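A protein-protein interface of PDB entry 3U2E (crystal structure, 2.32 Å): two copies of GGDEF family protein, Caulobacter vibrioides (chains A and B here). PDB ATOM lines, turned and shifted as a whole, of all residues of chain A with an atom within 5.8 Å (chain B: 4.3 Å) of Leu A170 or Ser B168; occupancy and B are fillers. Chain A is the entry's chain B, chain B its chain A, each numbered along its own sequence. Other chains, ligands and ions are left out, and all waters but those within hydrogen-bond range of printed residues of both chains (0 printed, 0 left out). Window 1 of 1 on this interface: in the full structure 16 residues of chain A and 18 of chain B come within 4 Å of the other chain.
The backbone carbonyl oxygen of Gly B166 sits at hydrogen-bond distance from the side-chain hydroxyl of Ser A171. O of Phe B167 lies within hydrogen-bond range of OG of Ser A169 (2.6 Å). The backbone carbonyl oxygen (O) of Phe B167 is in hydrogen-bond range of the backbone NH (N) of Leu A170 (3.5 Å). The backbone carbonyl oxygen (O) of Phe B167 is in hydrogen-bond range of the side-chain hydroxyl (OG) of Ser A171, at 3.0 Å. The backbone NH (N) of Leu A170 is in hydrogen-bond range of the backbone carbonyl oxygen (O) of Ser B168 (2.9 Å). OG of Ser B169 is in hydrogen-bond range of O of Phe A167, at 2.6 Å. The backbone carbonyl oxygen (O) of Ser A168 lies within hydrogen-bond range of the backbone NH (N) of Leu B170, at 3.0 Å.
The backbone NH (N) of Phe B167 lies within hydrogen-bond range of the side-chain carboxylate (OE2) of Glu B134. OE2 of Glu B134 sits at hydrogen-bond distance from N of Ser B168, at 2.6 Å. The side-chain carboxylate (OE1) of Glu B134 sits at hydrogen-bond distance from the backbone NH (N) of Ser B169 (2.7 Å). OG of Ser B168 sits at hydrogen-bond distance from O of Thr B165 (3.0 Å). OG of Ser A171 sits at hydrogen-bond distance from OG of Ser A169 (2.9 Å). O of Ser A171 is in hydrogen-bond range of OG1 of Thr A174 (2.8 Å).
O of Phe A167 touches N of Leu B170, at 3.5 Å. Ser A169 touches Ser B168. CD2 of Leu A170 touches OG of Ser B203, at 3.97 Å. Leu A170 touches Val B204 (CD1 to CG2, 3.9 Å). Leu A170 touches Leu B207 (CD1 to CD2, 3.9 Å). Ser A171 touches Gly B164 (CB to O, 3.5 Å). O of Gly B166 touches CE1 of Tyr A172 (3.3 Å). Phe B167 touches Tyr A172. Leu A207 touches Leu B170. CD1 of Leu A207 touches CB of Ser B203, 3.7 Å away.
Leu A170 touches just these residues of chain B: Phe B167 (3.5 Å), Ser B168 (2.9 Å), Ser B203 (3.97 Å), Val B204 (3.9 Å) and Leu B207 (3.9 Å). Ser B168 touches three residues of chain A. Of the printed residues of chain A, Leu B207 touches Leu A170 (3.9 Å). Of the printed residues of chain B, Ser A169 touches Phe B167 and Ser B168. Of the printed residues of chain A, Val B204 touches Leu A170 (3.9 Å). Printed residues of chain A within 4 Å of Ser B169: Phe A167 (2.6 Å) and Ser A168 (3.9 Å). Leu A173 touches none of the printed residues of chain B. Phe B163 touches none of the printed residues of chain A. The nearest residue of chain A that does not touch Ser B168 is Ser A168 (4.1 Å).
Hydrophobic or aromatic side chains of chain A that line the printed part of chain B: Leu A170, Tyr A172 and Leu A207. Of the 12 printed residues of chain B, 9 touch a printed residue of chain A. Hydrophobic or aromatic side chains of chain B within 4 Å of the printed part of chain A: Phe B167, Leu B170, Val B204 and Leu B207. Among the printed residues, 19 pairs touch across the chains. Among the printed residues, no Asp or Glu carboxylate lies within 4 Å of a Lys or Arg side-chain nitrogen of the other chain.
Phe A167 touches Leu B170, and with the chains exchanged Leu A170 touches Phe B167. Ser A168 touches Ser B169, and with the chains exchanged Ser A169 touches Ser B168. Ser A168 touches Leu B170, and with the chains exchanged Leu A170 touches Ser B168. Leu A170 touches Leu B207, and with the chains exchanged Leu A207 touches Leu B170. Of the 19 pairs that touch across the chains among the printed residues, 10 have their exchanged pair printed and touching as well.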
ATOM      1  N   PHE A 163     -24.175  25.058  16.919  1.00  0.00           N
ATOM      2  CA  PHE A 163     -23.713  23.786  17.395  1.00  0.00           C
ATOM      3  C   PHE A 163     -24.775  23.173  18.310  1.00  0.00           C
ATOM      4  O   PHE A 163     -25.411  23.853  19.113  1.00  0.00           O
ATOM      5  CB  PHE A 163     -22.357  23.890  18.087  1.00  0.00           C
ATOM      6  CG  PHE A 163     -21.619  22.598  18.147  1.00  0.00           C
ATOM      7  CD1 PHE A 163     -20.980  22.099  17.020  1.00  0.00           C
ATOM      8  CD2 PHE A 163     -21.538  21.868  19.315  1.00  0.00           C
ATOM      9  CE1 PHE A 163     -20.267  20.875  17.054  1.00  0.00           C
ATOM     10  CE2 PHE A 163     -20.822  20.649  19.370  1.00  0.00           C
ATOM     11  CZ  PHE A 163     -20.196  20.157  18.233  1.00  0.00           C
ATOM     12  N   PHE A 167     -25.321  16.905  13.216  1.00  0.00           N
ATOM     13  CA  PHE A 167     -24.387  15.900  13.746  1.00  0.00           C
ATOM     14  C   PHE A 167     -23.612  16.332  14.973  1.00  0.00           C
ATOM     15  O   PHE A 167     -23.474  15.553  15.921  1.00  0.00           O
ATOM     16  CB  PHE A 167     -23.440  15.437  12.655  1.00  0.00           C
ATOM     17  CG  PHE A 167     -24.133  14.814  11.480  1.00  0.00           C
ATOM     18  CD1 PHE A 167     -24.685  13.551  11.580  1.00  0.00           C
ATOM     19  CD2 PHE A 167     -24.238  15.504  10.267  1.00  0.00           C
ATOM     20  CE1 PHE A 167     -25.320  12.955  10.486  1.00  0.00           C
ATOM     21  CE2 PHE A 167     -24.876  14.933   9.175  1.00  0.00           C
ATOM     22  CZ  PHE A 167     -25.424  13.647   9.281  1.00  0.00           C
ATOM     23  N   SER A 168     -23.184  17.595  14.990  1.00  0.00           N
ATOM     24  CA  SER A 168     -22.405  18.117  16.094  1.00  0.00           C
ATOM     25  C   SER A 168     -21.272  17.115  16.383  1.00  0.00           C
ATOM     26  O   SER A 168     -21.159  16.565  17.512  1.00  0.00           O
ATOM     27  CB  SER A 168     -23.301  18.345  17.309  1.00  0.00           C
ATOM     28  OG  SER A 168     -24.294  19.354  17.053  1.00  0.00           O
ATOM     29  N   SER A 169     -20.476  16.850  15.344  1.00  0.00           N
ATOM     30  CA  SER A 169     -19.389  15.865  15.394  1.00  0.00           C
ATOM     31  C   SER A 169     -18.249  16.177  16.337  1.00  0.00           C
ATOM     32  O   SER A 169     -17.601  17.180  16.169  1.00  0.00           O
ATOM     33  CB  SER A 169     -18.777  15.731  14.021  1.00  0.00           C
ATOM     34  OG  SER A 169     -17.593  14.973  14.099  1.00  0.00           O
ATOM     35  N   LEU A 170     -17.991  15.316  17.327  1.00  0.00           N
ATOM     36  CA  LEU A 170     -16.873  15.556  18.249  1.00  0.00           C
ATOM     37  C   LEU A 170     -15.523  15.279  17.569  1.00  0.00           C
ATOM     38  O   LEU A 170     -14.551  15.967  17.808  1.00  0.00           O
ATOM     39  CB  LEU A 170     -17.045  14.721  19.490  1.00  0.00           C
ATOM     40  CG  LEU A 170     -15.912  14.497  20.472  1.00  0.00           C
ATOM     41  CD1 LEU A 170     -16.502  13.746  21.673  1.00  0.00           C
ATOM     42  CD2 LEU A 170     -14.755  13.717  19.854  1.00  0.00           C
ATOM     43  N   SER A 171     -15.488  14.318  16.664  1.00  0.00           N
ATOM     44  CA  SER A 171     -14.267  13.990  15.948  1.00  0.00           C
ATOM     45  C   SER A 171     -13.829  15.097  14.974  1.00  0.00           C
ATOM     46  O   SER A 171     -12.698  15.583  15.032  1.00  0.00           O
ATOM     47  CB  SER A 171     -14.475  12.689  15.203  1.00  0.00           C
ATOM     48  OG  SER A 171     -15.677  12.774  14.429  1.00  0.00           O
ATOM     49  N   TYR A 172     -14.723  15.505  14.086  1.00  0.00           N
ATOM     50  CA  TYR A 172     -14.394  16.561  13.089  1.00  0.00           C
ATOM     51  C   TYR A 172     -13.950  17.838  13.795  1.00  0.00           C
ATOM     52  O   TYR A 172     -12.991  18.464  13.425  1.00  0.00           O
ATOM     53  CB  TYR A 172     -15.592  16.827  12.189  1.00  0.00           C
ATOM     54  CG  TYR A 172     -15.856  15.740  11.170  1.00  0.00           C
ATOM     55  CD1 TYR A 172     -15.625  14.420  11.462  1.00  0.00           C
ATOM     56  CD2 TYR A 172     -16.441  16.035   9.942  1.00  0.00           C
ATOM     57  CE1 TYR A 172     -15.873  13.427  10.537  1.00  0.00           C
ATOM     58  CE2 TYR A 172     -16.722  15.040   9.024  1.00  0.00           C
ATOM     59  CZ  TYR A 172     -16.435  13.735   9.333  1.00  0.00           C
ATOM     60  OH  TYR A 172     -16.695  12.710   8.442  1.00  0.00           O
ATOM     61  N   LEU A 173     -14.593  18.165  14.888  1.00  0.00           N
ATOM     62  CA  LEU A 173     -14.240  19.360  15.597  1.00  0.00           C
ATOM     63  C   LEU A 173     -12.783  19.405  16.013  1.00  0.00           C
ATOM     64  O   LEU A 173     -12.138  20.433  15.859  1.00  0.00           O
ATOM     65  CB  LEU A 173     -15.129  19.494  16.820  1.00  0.00           C
ATOM     66  CG  LEU A 173     -15.119  20.845  17.480  1.00  0.00           C
ATOM     67  CD1 LEU A 173     -15.404  21.929  16.425  1.00  0.00           C
ATOM     68  CD2 LEU A 173     -16.149  20.851  18.597  1.00  0.00           C
ATOM     69  N   THR A 174     -12.247  18.280  16.492  1.00  0.00           N
ATOM     70  CA  THR A 174     -10.876  18.245  17.012  1.00  0.00           C
ATOM     71  C   THR A 174      -9.832  18.511  15.973  1.00  0.00           C
ATOM     72  O   THR A 174      -8.683  18.652  16.303  1.00  0.00           O
ATOM     73  CB  THR A 174     -10.501  16.883  17.647  1.00  0.00           C
ATOM     74  OG1 THR A 174     -10.445  15.867  16.638  1.00  0.00           O
ATOM     75  CG2 THR A 174     -11.443  16.484  18.715  1.00  0.00           C
ATOM     76  N   LEU A 207     -17.468  20.150  26.402  1.00  0.00           N
ATOM     77  CA  LEU A 207     -16.665  19.814  25.247  1.00  0.00           C
ATOM     78  C   LEU A 207     -15.777  20.983  24.859  1.00  0.00           C
ATOM     79  O   LEU A 207     -14.620  20.791  24.532  1.00  0.00           O
ATOM     80  CB  LEU A 207     -17.576  19.483  24.075  1.00  0.00           C
ATOM     81  CG  LEU A 207     -16.818  19.143  22.820  1.00  0.00           C
ATOM     82  CD1 LEU A 207     -16.058  17.839  23.011  1.00  0.00           C
ATOM     83  CD2 LEU A 207     -17.782  19.072  21.641  1.00  0.00           C
ATOM     84  N   LEU A 211     -11.725  21.069  24.670  1.00  0.00           N
ATOM     85  CA  LEU A 211     -11.034  21.341  23.429  1.00  0.00           C
ATOM     86  C   LEU A 211     -10.423  22.730  23.390  1.00  0.00           C
ATOM     87  O   LEU A 211      -9.811  23.080  22.406  1.00  0.00           O
ATOM     88  CB  LEU A 211     -11.960  21.147  22.236  1.00  0.00           C
ATOM     89  CG  LEU A 211     -12.564  19.763  22.057  1.00  0.00           C
ATOM     90  CD1 LEU A 211     -13.516  19.780  20.869  1.00  0.00           C
ATOM     91  CD2 LEU A 211     -11.444  18.759  21.876  1.00  0.00           C
ATOM     92  N   GLU B 134     -21.512   3.198  15.398  1.00  0.00           N
ATOM     93  CA  GLU B 134     -22.221   4.431  15.101  1.00  0.00           C
ATOM     94  C   GLU B 134     -22.747   4.432  13.658  1.00  0.00           C
ATOM     95  O   GLU B 134     -23.784   4.986  13.395  1.00  0.00           O
ATOM     96  CB  GLU B 134     -21.332   5.664  15.361  1.00  0.00           C
ATOM     97  CG  GLU B 134     -22.147   6.954  15.395  1.00  0.00           C
ATOM     98  CD  GLU B 134     -21.337   8.247  15.501  1.00  0.00           C
ATOM     99  OE1 GLU B 134     -21.926   9.227  16.026  1.00  0.00           O
ATOM    100  OE2 GLU B 134     -20.155   8.308  15.024  1.00  0.00           O
ATOM    101  N   PHE B 163     -16.255   4.411  19.412  1.00  0.00           N
ATOM    102  CA  PHE B 163     -16.555   5.803  19.390  1.00  0.00           C
ATOM    103  C   PHE B 163     -15.247   6.555  19.169  1.00  0.00           C
ATOM    104  O   PHE B 163     -14.171   6.090  19.581  1.00  0.00           O
ATOM    105  CB  PHE B 163     -17.266   6.234  20.653  1.00  0.00           C
ATOM    106  CG  PHE B 163     -18.013   7.534  20.492  1.00  0.00           C
ATOM    107  CD1 PHE B 163     -19.194   7.568  19.787  1.00  0.00           C
ATOM    108  CD2 PHE B 163     -17.538   8.707  21.046  1.00  0.00           C
ATOM    109  CE1 PHE B 163     -19.918   8.741  19.658  1.00  0.00           C
ATOM    110  CE2 PHE B 163     -18.251   9.890  20.918  1.00  0.00           C
ATOM    111  CZ  PHE B 163     -19.426   9.917  20.189  1.00  0.00           C
ATOM    112  N   GLY B 164     -15.342   7.695  18.479  1.00  0.00           N
ATOM    113  CA  GLY B 164     -14.167   8.498  18.147  1.00  0.00           C
ATOM    114  C   GLY B 164     -13.973   8.488  16.649  1.00  0.00           C
ATOM    115  O   GLY B 164     -13.488   9.466  16.062  1.00  0.00           O
ATOM    116  N   THR B 165     -14.350   7.379  16.029  1.00  0.00           N
ATOM    117  CA  THR B 165     -14.258   7.259  14.589  1.00  0.00           C
ATOM    118  C   THR B 165     -15.489   7.925  13.984  1.00  0.00           C
ATOM    119  O   THR B 165     -16.455   8.281  14.686  1.00  0.00           O
ATOM    120  CB  THR B 165     -14.236   5.763  14.106  1.00  0.00           C
ATOM    121  OG1 THR B 165     -15.443   5.095  14.518  1.00  0.00           O
ATOM    122  CG2 THR B 165     -13.023   4.996  14.666  1.00  0.00           C
ATOM    123  N   GLY B 166     -15.444   8.101  12.674  1.00  0.00           N
ATOM    124  CA  GLY B 166     -16.572   8.637  11.932  1.00  0.00           C
ATOM    125  C   GLY B 166     -17.025   9.987  12.435  1.00  0.00           C
ATOM    126  O   GLY B 166     -16.219  10.874  12.632  1.00  0.00           O
ATOM    127  N   PHE B 167     -18.319  10.090  12.692  1.00  0.00           N
ATOM    128  CA  PHE B 167     -18.940  11.320  13.153  1.00  0.00           C
ATOM    129  C   PHE B 167     -18.821  11.599  14.645  1.00  0.00           C
ATOM    130  O   PHE B 167     -18.663  12.771  15.023  1.00  0.00           O
ATOM    131  CB  PHE B 167     -20.428  11.341  12.780  1.00  0.00           C
ATOM    132  CG  PHE B 167     -20.677  11.221  11.313  1.00  0.00           C
ATOM    133  CD1 PHE B 167     -20.167  12.160  10.441  1.00  0.00           C
ATOM    134  CD2 PHE B 167     -21.453  10.196  10.811  1.00  0.00           C
ATOM    135  CE1 PHE B 167     -20.405  12.072   9.084  1.00  0.00           C
ATOM    136  CE2 PHE B 167     -21.704  10.099   9.449  1.00  0.00           C
ATOM    137  CZ  PHE B 167     -21.175  11.042   8.584  1.00  0.00           C
ATOM    138  N   SER B 168     -18.889  10.543  15.471  1.00  0.00           N
ATOM    139  CA  SER B 168     -18.865  10.691  16.912  1.00  0.00           C
ATOM    140  C   SER B 168     -19.839  11.829  17.290  1.00  0.00           C
ATOM    141  O   SER B 168     -19.437  12.827  17.900  1.00  0.00           O
ATOM    142  CB  SER B 168     -17.446  11.009  17.387  1.00  0.00           C
ATOM    143  OG  SER B 168     -16.568   9.906  17.187  1.00  0.00           O
ATOM    144  N   SER B 169     -21.092  11.676  16.855  1.00  0.00           N
ATOM    145  CA  SER B 169     -22.115  12.672  17.045  1.00  0.00           C
ATOM    146  C   SER B 169     -22.435  12.961  18.492  1.00  0.00           C
ATOM    147  O   SER B 169     -22.869  12.074  19.212  1.00  0.00           O
ATOM    148  CB  SER B 169     -23.380  12.230  16.373  1.00  0.00           C
ATOM    149  OG  SER B 169     -24.370  13.197  16.574  1.00  0.00           O
ATOM    150  N   LEU B 170     -22.225  14.191  18.932  1.00  0.00           N
ATOM    151  CA  LEU B 170     -22.573  14.552  20.327  1.00  0.00           C
ATOM    152  C   LEU B 170     -24.078  14.630  20.459  1.00  0.00           C
ATOM    153  O   LEU B 170     -24.628  14.093  21.410  1.00  0.00           O
ATOM    154  CB  LEU B 170     -21.917  15.859  20.774  1.00  0.00           C
ATOM    155  CG  LEU B 170     -22.356  16.581  22.061  1.00  0.00           C
ATOM    156  CD1 LEU B 170     -21.235  17.479  22.586  1.00  0.00           C
ATOM    157  CD2 LEU B 170     -23.645  17.384  21.890  1.00  0.00           C
ATOM    158  N   SER B 203     -11.984  14.007  25.559  1.00  0.00           N
ATOM    159  CA  SER B 203     -13.326  14.560  25.476  1.00  0.00           C
ATOM    160  C   SER B 203     -14.390  13.482  25.391  1.00  0.00           C
ATOM    161  O   SER B 203     -15.508  13.689  25.857  1.00  0.00           O
ATOM    162  CB  SER B 203     -13.409  15.614  24.363  1.00  0.00           C
ATOM    163  OG  SER B 203     -12.982  15.091  23.126  1.00  0.00           O
ATOM    164  N   VAL B 204     -14.060  12.312  24.848  1.00  0.00           N
ATOM    165  CA  VAL B 204     -15.033  11.227  24.860  1.00  0.00           C
ATOM    166  C   VAL B 204     -15.266  10.772  26.303  1.00  0.00           C
ATOM    167  O   VAL B 204     -16.386  10.532  26.689  1.00  0.00           O
ATOM    168  CB  VAL B 204     -14.614  10.031  24.005  1.00  0.00           C
ATOM    169  CG1 VAL B 204     -15.536   8.845  24.264  1.00  0.00           C
ATOM    170  CG2 VAL B 204     -14.569  10.415  22.532  1.00  0.00           C
ATOM    171  N   LEU B 207     -17.445  13.507  28.043  1.00  0.00           N
ATOM    172  CA  LEU B 207     -18.766  13.462  27.438  1.00  0.00           C
ATOM    173  C   LEU B 207     -19.514  12.203  27.929  1.00  0.00           C
ATOM    174  O   LEU B 207     -20.691  12.243  28.290  1.00  0.00           O
ATOM    175  CB  LEU B 207     -18.629  13.410  25.913  1.00  0.00           C
ATOM    176  CG  LEU B 207     -19.936  13.196  25.144  1.00  0.00           C
ATOM    177  CD1 LEU B 207     -20.854  14.393  25.339  1.00  0.00           C
ATOM    178  CD2 LEU B 207     -19.718  12.924  23.660  1.00  0.00           C
